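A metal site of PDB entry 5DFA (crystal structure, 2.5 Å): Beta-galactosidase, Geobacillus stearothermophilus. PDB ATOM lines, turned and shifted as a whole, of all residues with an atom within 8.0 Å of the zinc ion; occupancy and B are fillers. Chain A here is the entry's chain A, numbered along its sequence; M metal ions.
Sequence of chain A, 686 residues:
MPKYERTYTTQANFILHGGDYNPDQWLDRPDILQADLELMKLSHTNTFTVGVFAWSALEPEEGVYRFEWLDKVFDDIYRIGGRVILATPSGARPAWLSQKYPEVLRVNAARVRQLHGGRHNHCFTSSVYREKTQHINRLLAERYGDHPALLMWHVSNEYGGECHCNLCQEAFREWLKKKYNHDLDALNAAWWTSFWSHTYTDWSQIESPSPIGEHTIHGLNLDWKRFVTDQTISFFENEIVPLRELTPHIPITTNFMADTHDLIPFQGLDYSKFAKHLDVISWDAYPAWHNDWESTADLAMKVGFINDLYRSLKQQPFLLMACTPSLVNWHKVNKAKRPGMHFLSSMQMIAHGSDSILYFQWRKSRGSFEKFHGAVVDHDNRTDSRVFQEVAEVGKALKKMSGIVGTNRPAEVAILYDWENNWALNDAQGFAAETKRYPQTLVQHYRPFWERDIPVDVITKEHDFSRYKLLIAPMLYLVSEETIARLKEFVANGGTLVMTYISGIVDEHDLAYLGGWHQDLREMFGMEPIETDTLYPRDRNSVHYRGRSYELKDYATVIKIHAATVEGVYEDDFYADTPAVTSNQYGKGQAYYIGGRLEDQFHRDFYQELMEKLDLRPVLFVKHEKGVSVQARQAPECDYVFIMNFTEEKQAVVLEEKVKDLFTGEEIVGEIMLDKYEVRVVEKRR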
ATOM      1  N   GLU A 103       4.925  30.847  23.225  1.00  0.00           N
ATOM      2  CA  GLU A 103       4.448  30.020  24.334  1.00  0.00           C
ATOM      3  C   GLU A 103       2.967  29.674  24.198  1.00  0.00           C
ATOM      4  O   GLU A 103       2.448  28.839  24.936  1.00  0.00           O
ATOM      5  CB  GLU A 103       4.705  30.712  25.676  1.00  0.00           C
ATOM      6  CG  GLU A 103       3.853  31.943  25.920  1.00  0.00           C
ATOM      7  CD  GLU A 103       3.754  32.294  27.396  1.00  0.00           C
ATOM      8  OE1 GLU A 103       4.811  32.371  28.060  1.00  0.00           O
ATOM      9  OE2 GLU A 103       2.625  32.474  27.887  1.00  0.00           O
ATOM     10  N   VAL A 104       2.292  30.323  23.251  1.00  0.00           N
ATOM     11  CA  VAL A 104       0.870  30.054  23.022  1.00  0.00           C
ATOM     12  C   VAL A 104       0.694  28.826  22.127  1.00  0.00           C
ATOM     13  O   VAL A 104      -0.411  28.327  21.959  1.00  0.00           O
ATOM     14  CB  VAL A 104       0.162  31.259  22.376  1.00  0.00           C
ATOM     15  CG1 VAL A 104       0.413  32.519  23.195  1.00  0.00           C
ATOM     16  CG2 VAL A 104       0.622  31.443  20.943  1.00  0.00           C
ATOM     17  N   LEU A 105       1.797  28.358  21.544  1.00  0.00           N
ATOM     18  CA  LEU A 105       1.769  27.178  20.692  1.00  0.00           C
ATOM     19  C   LEU A 105       1.737  25.904  21.518  1.00  0.00           C
ATOM     20  O   LEU A 105       2.367  25.817  22.572  1.00  0.00           O
ATOM     21  CB  LEU A 105       2.972  27.179  19.746  1.00  0.00           C
ATOM     22  CG  LEU A 105       2.928  28.214  18.618  1.00  0.00           C
ATOM     23  CD1 LEU A 105       4.256  28.280  17.895  1.00  0.00           C
ATOM     24  CD2 LEU A 105       1.807  27.893  17.650  1.00  0.00           C
ATOM     25  N   ARG A 106       1.012  24.904  21.024  1.00  0.00           N
ATOM     26  CA  ARG A 106       0.820  23.657  21.760  1.00  0.00           C
ATOM     27  C   ARG A 106       2.021  22.725  21.696  1.00  0.00           C
ATOM     28  O   ARG A 106       2.842  22.793  20.777  1.00  0.00           O
ATOM     29  CB  ARG A 106      -0.397  22.911  21.216  1.00  0.00           C
ATOM     30  CG  ARG A 106      -1.698  23.239  21.917  1.00  0.00           C
ATOM     31  CD  ARG A 106      -2.807  22.308  21.432  1.00  0.00           C
ATOM     32  NE  ARG A 106      -4.099  22.650  22.010  1.00  0.00           N
ATOM     33  CZ  ARG A 106      -5.260  22.197  21.550  1.00  0.00           C
ATOM     34  NH1 ARG A 106      -5.287  21.365  20.509  1.00  0.00           N
ATOM     35  NH2 ARG A 106      -6.395  22.551  22.138  1.00  0.00           N
ATOM     36  N   VAL A 107       2.108  21.861  22.699  1.00  0.00           N
ATOM     37  CA  VAL A 107       3.028  20.737  22.689  1.00  0.00           C
ATOM     38  C   VAL A 107       2.200  19.460  22.830  1.00  0.00           C
ATOM     39  O   VAL A 107       1.541  19.254  23.851  1.00  0.00           O
ATOM     40  CB  VAL A 107       4.054  20.825  23.842  1.00  0.00           C
ATOM     41  CG1 VAL A 107       4.873  19.563  23.918  1.00  0.00           C
ATOM     42  CG2 VAL A 107       4.951  22.034  23.647  1.00  0.00           C
ATOM     43  N   ARG A 113       6.593  20.331  19.945  1.00  0.00           N
ATOM     44  CA  ARG A 113       6.054  21.678  19.840  1.00  0.00           C
ATOM     45  C   ARG A 113       5.450  21.902  18.449  1.00  0.00           C
ATOM     46  O   ARG A 113       6.090  21.632  17.431  1.00  0.00           O
ATOM     47  CB  ARG A 113       7.133  22.725  20.116  1.00  0.00           C
ATOM     48  CG  ARG A 113       6.650  24.164  19.981  1.00  0.00           C
ATOM     49  CD  ARG A 113       5.822  24.594  21.179  1.00  0.00           C
ATOM     50  NE  ARG A 113       6.616  24.675  22.393  1.00  0.00           N
ATOM     51  CZ  ARG A 113       6.207  25.238  23.535  1.00  0.00           C
ATOM     52  NH1 ARG A 113       5.001  25.783  23.601  1.00  0.00           N
ATOM     53  NH2 ARG A 113       7.003  25.260  24.594  1.00  0.00           N
ATOM     54  N   HIS A 122      -4.523  26.190  20.909  1.00  0.00           N
ATOM     55  CA  HIS A 122      -3.715  27.061  21.758  1.00  0.00           C
ATOM     56  C   HIS A 122      -3.334  26.363  23.052  1.00  0.00           C
ATOM     57  O   HIS A 122      -3.991  25.411  23.475  1.00  0.00           O
ATOM     58  CB  HIS A 122      -4.468  28.358  22.073  1.00  0.00           C
ATOM     59  CG  HIS A 122      -5.702  28.151  22.884  1.00  0.00           C
ATOM     60  ND1 HIS A 122      -6.907  27.794  22.332  1.00  0.00           N
ATOM     61  CD2 HIS A 122      -5.919  28.258  24.225  1.00  0.00           C
ATOM     62  CE1 HIS A 122      -7.822  27.687  23.285  1.00  0.00           C
ATOM     63  NE2 HIS A 122      -7.249  27.964  24.442  1.00  0.00           N
ATOM     64  N   CYS A 123      -2.258  26.836  23.684  1.00  0.00           N
ATOM     65  CA  CYS A 123      -1.896  26.368  25.017  1.00  0.00           C
ATOM     66  C   CYS A 123      -2.854  26.977  26.038  1.00  0.00           C
ATOM     67  O   CYS A 123      -2.907  28.195  26.201  1.00  0.00           O
ATOM     68  CB  CYS A 123      -0.447  26.741  25.342  1.00  0.00           C
ATOM     69  SG  CYS A 123       0.017  26.499  27.077  1.00  0.00           S
ATOM     70  N   PHE A 124      -3.614  26.125  26.718  1.00  0.00           N
ATOM     71  CA  PHE A 124      -4.663  26.608  27.612  1.00  0.00           C
ATOM     72  C   PHE A 124      -4.127  27.015  28.986  1.00  0.00           C
ATOM     73  O   PHE A 124      -4.896  27.381  29.875  1.00  0.00           O
ATOM     74  CB  PHE A 124      -5.761  25.556  27.773  1.00  0.00           C
ATOM     75  CG  PHE A 124      -5.256  24.190  28.141  1.00  0.00           C
ATOM     76  CD1 PHE A 124      -4.921  23.892  29.454  1.00  0.00           C
ATOM     77  CD2 PHE A 124      -5.147  23.183  27.192  1.00  0.00           C
ATOM     78  CE1 PHE A 124      -4.472  22.639  29.811  1.00  0.00           C
ATOM     79  CE2 PHE A 124      -4.698  21.931  27.550  1.00  0.00           C
ATOM     80  CZ  PHE A 124      -4.363  21.656  28.856  1.00  0.00           C
ATOM     81  N   THR A 125      -2.802  26.950  29.164  1.00  0.00           N
ATOM     82  CA  THR A 125      -2.184  27.380  30.406  1.00  0.00           C
ATOM     83  C   THR A 125      -1.527  28.747  30.243  1.00  0.00           C
ATOM     84  O   THR A 125      -1.577  29.579  31.152  1.00  0.00           O
ATOM     85  CB  THR A 125      -1.132  26.366  30.901  1.00  0.00           C
ATOM     86  OG1 THR A 125      -1.748  25.109  31.176  1.00  0.00           O
ATOM     87  CG2 THR A 125      -0.441  26.862  32.169  1.00  0.00           C
ATOM     88  N   SER A 126      -0.941  28.959  29.066  1.00  0.00           N
ATOM     89  CA  SER A 126      -0.175  30.169  28.741  1.00  0.00           C
ATOM     90  C   SER A 126      -0.793  31.458  29.280  1.00  0.00           C
ATOM     91  O   SER A 126      -1.886  31.855  28.887  1.00  0.00           O
ATOM     92  CB  SER A 126      -0.018  30.277  27.223  1.00  0.00           C
ATOM     93  OG  SER A 126       0.565  31.522  26.860  1.00  0.00           O
ATOM     94  N   GLU A 162      -5.562  19.354  23.836  1.00  0.00           N
ATOM     95  CA  GLU A 162      -4.792  19.479  25.069  1.00  0.00           C
ATOM     96  C   GLU A 162      -3.352  19.887  24.783  1.00  0.00           C
ATOM     97  O   GLU A 162      -2.879  19.787  23.652  1.00  0.00           O
ATOM     98  CB  GLU A 162      -4.834  18.160  25.839  1.00  0.00           C
ATOM     99  CG  GLU A 162      -4.491  16.939  25.003  1.00  0.00           C
ATOM    100  CD  GLU A 162      -4.802  15.630  25.707  1.00  0.00           C
ATOM    101  OE1 GLU A 162      -5.946  15.472  26.177  1.00  0.00           O
ATOM    102  OE2 GLU A 162      -3.901  14.770  25.779  1.00  0.00           O
ATOM    103  N   CYS A 163      -2.669  20.361  25.822  1.00  0.00           N
ATOM    104  CA  CYS A 163      -1.275  20.758  25.695  1.00  0.00           C
ATOM    105  C   CYS A 163      -0.444  20.073  26.773  1.00  0.00           C
ATOM    106  O   CYS A 163      -0.919  19.843  27.882  1.00  0.00           O
ATOM    107  CB  CYS A 163      -1.134  22.276  25.804  1.00  0.00           C
ATOM    108  SG  CYS A 163       0.540  22.880  25.460  1.00  0.00           S
ATOM    109  N   HIS A 164       0.800  19.745  26.437  1.00  0.00           N
ATOM    110  CA  HIS A 164       1.678  19.034  27.359  1.00  0.00           C
ATOM    111  C   HIS A 164       2.983  19.786  27.588  1.00  0.00           C
ATOM    112  O   HIS A 164       3.985  19.177  27.978  1.00  0.00           O
ATOM    113  CB  HIS A 164       1.981  17.624  26.829  1.00  0.00           C
ATOM    114  CG  HIS A 164       0.751  16.806  26.570  1.00  0.00           C
ATOM    115  ND1 HIS A 164       0.305  15.833  27.435  1.00  0.00           N
ATOM    116  CD2 HIS A 164      -0.115  16.809  25.532  1.00  0.00           C
ATOM    117  CE1 HIS A 164      -0.784  15.270  26.942  1.00  0.00           C
ATOM    118  NE2 HIS A 164      -1.060  15.845  25.785  1.00  0.00           N
ATOM    119  N   CYS A 165       2.978  21.089  27.357  1.00  0.00           N
ATOM    120  CA  CYS A 165       4.180  21.898  27.553  1.00  0.00           C
ATOM    121  C   CYS A 165       4.536  21.986  29.033  1.00  0.00           C
ATOM    122  O   CYS A 165       3.745  21.592  29.891  1.00  0.00           O
ATOM    123  CB  CYS A 165       3.997  23.305  26.975  1.00  0.00           C
ATOM    124  SG  CYS A 165       3.044  24.433  28.022  1.00  0.00           S
ATOM    125  N   ASN A 166       5.721  22.494  29.323  1.00  0.00           N
ATOM    126  CA  ASN A 166       6.224  22.622  30.690  1.00  0.00           C
ATOM    127  C   ASN A 166       5.289  23.405  31.596  1.00  0.00           C
ATOM    128  O   ASN A 166       5.154  23.104  32.785  1.00  0.00           O
ATOM    129  CB  ASN A 166       7.603  23.313  30.675  1.00  0.00           C
ATOM    130  CG  ASN A 166       7.558  24.678  30.022  1.00  0.00           C
ATOM    131  OD1 ASN A 166       6.980  24.862  28.952  1.00  0.00           O
ATOM    132  ND2 ASN A 166       8.171  25.660  30.678  1.00  0.00           N
ATOM    133  N   LEU A 167       4.652  24.428  31.045  1.00  0.00           N
ATOM    134  CA  LEU A 167       3.723  25.252  31.803  1.00  0.00           C
ATOM    135  C   LEU A 167       2.512  24.423  32.218  1.00  0.00           C
ATOM    136  O   LEU A 167       2.028  24.515  33.349  1.00  0.00           O
ATOM    137  CB  LEU A 167       3.271  26.469  30.986  1.00  0.00           C
ATOM    138  CG  LEU A 167       4.376  27.433  30.543  1.00  0.00           C
ATOM    139  CD1 LEU A 167       3.807  28.536  29.665  1.00  0.00           C
ATOM    140  CD2 LEU A 167       5.095  28.011  31.748  1.00  0.00           C
ATOM    141  N   CYS A 168       2.021  23.600  31.293  1.00  0.00           N
ATOM    142  CA  CYS A 168       0.884  22.730  31.563  1.00  0.00           C
ATOM    143  C   CYS A 168       1.259  21.605  32.524  1.00  0.00           C
ATOM    144  O   CYS A 168       0.430  21.156  33.322  1.00  0.00           O
ATOM    145  CB  CYS A 168       0.341  22.140  30.259  1.00  0.00           C
ATOM    146  SG  CYS A 168      -0.539  23.322  29.216  1.00  0.00           S
ATOM    147  N   GLN A 169       2.511  21.154  32.447  1.00  0.00           N
ATOM    148  CA  GLN A 169       3.000  20.101  33.329  1.00  0.00           C
ATOM    149  C   GLN A 169       2.953  20.548  34.788  1.00  0.00           C
ATOM    150  O   GLN A 169       2.478  19.819  35.656  1.00  0.00           O
ATOM    151  CB  GLN A 169       4.419  19.677  32.943  1.00  0.00           C
ATOM    152  CG  GLN A 169       4.536  19.002  31.592  1.00  0.00           C
ATOM    153  CD  GLN A 169       3.743  17.717  31.494  1.00  0.00           C
ATOM    154  OE1 GLN A 169       3.526  17.027  32.494  1.00  0.00           O
ATOM    155  NE2 GLN A 169       3.302  17.368  30.292  1.00  0.00           N
ATOM    156  N   ALA A 171       1.221  23.062  35.904  1.00  0.00           N
ATOM    157  CA  ALA A 171      -0.172  23.356  36.200  1.00  0.00           C
ATOM    158  C   ALA A 171      -0.903  22.074  36.600  1.00  0.00           C
ATOM    159  O   ALA A 171      -1.772  22.084  37.477  1.00  0.00           O
ATOM    160  CB  ALA A 171      -0.851  24.002  35.003  1.00  0.00           C
ATOM    161  N   TRP A 224      -5.779  13.140  34.204  1.00  0.00           N
ATOM    162  CA  TRP A 224      -5.282  14.046  33.175  1.00  0.00           C
ATOM    163  C   TRP A 224      -6.444  14.617  32.364  1.00  0.00           C
ATOM    164  O   TRP A 224      -6.491  15.822  32.100  1.00  0.00           O
ATOM    165  CB  TRP A 224      -4.301  13.333  32.235  1.00  0.00           C
ATOM    166  CG  TRP A 224      -3.907  14.154  31.048  1.00  0.00           C
ATOM    167  CD1 TRP A 224      -4.219  13.907  29.747  1.00  0.00           C
ATOM    168  CD2 TRP A 224      -3.150  15.370  31.053  1.00  0.00           C
ATOM    169  NE1 TRP A 224      -3.696  14.882  28.937  1.00  0.00           N
ATOM    170  CE2 TRP A 224      -3.030  15.790  29.718  1.00  0.00           C
ATOM    171  CE3 TRP A 224      -2.550  16.126  32.062  1.00  0.00           C
ATOM    172  CZ2 TRP A 224      -2.340  16.947  29.369  1.00  0.00           C
ATOM    173  CZ3 TRP A 224      -1.864  17.277  31.706  1.00  0.00           C
ATOM    174  CH2 TRP A 224      -1.767  17.681  30.371  1.00  0.00           C
ATOM    175  N   PHE A 227      -8.175  17.150  34.407  1.00  0.00           N
ATOM    176  CA  PHE A 227      -7.400  18.389  34.409  1.00  0.00           C
ATOM    177  C   PHE A 227      -7.603  19.177  33.114  1.00  0.00           C
ATOM    178  O   PHE A 227      -7.738  20.403  33.141  1.00  0.00           O
ATOM    179  CB  PHE A 227      -5.916  18.095  34.612  1.00  0.00           C
ATOM    180  CG  PHE A 227      -5.014  19.250  34.298  1.00  0.00           C
ATOM    181  CD1 PHE A 227      -4.869  20.295  35.188  1.00  0.00           C
ATOM    182  CD2 PHE A 227      -4.315  19.296  33.100  1.00  0.00           C
ATOM    183  CE1 PHE A 227      -4.046  21.365  34.897  1.00  0.00           C
ATOM    184  CE2 PHE A 227      -3.488  20.362  32.795  1.00  0.00           C
ATOM    185  CZ  PHE A 227      -3.357  21.402  33.699  1.00  0.00           C
HETATM  186 ZN    ZN M   1       0.767  24.201  27.422  1.00  0.00          ZN
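SG of Cys 123 lies close to N of Ser 126, 3.3 Å away.
N of Cys 123 lies within hydrogen-bond range of O of Val 104, 2.9 Å away.
SG of Cys 163 lies close to N of Val 107 (3.3 Å).
N of Leu 167 lies close to SG of Cys 165 (3.4 Å).
The side-chain sulfur of Cys 123 lies close to the backbone NH of Thr 125.
The side-chain sulfur (SG) of Cys 168 sits close to the side-chain hydroxyl (OG1) of Thr 125 (2.9 Å).
Within 4 Å of the zinc ion: Cys 123, Cys 163, Cys 165 and Cys 168.
The zinc ion is bound by SG of Cys 165, SG of Cys 163, SG of Cys 168 and SG of Cys 123.
The zinc ion has four donor atoms within binding distance.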
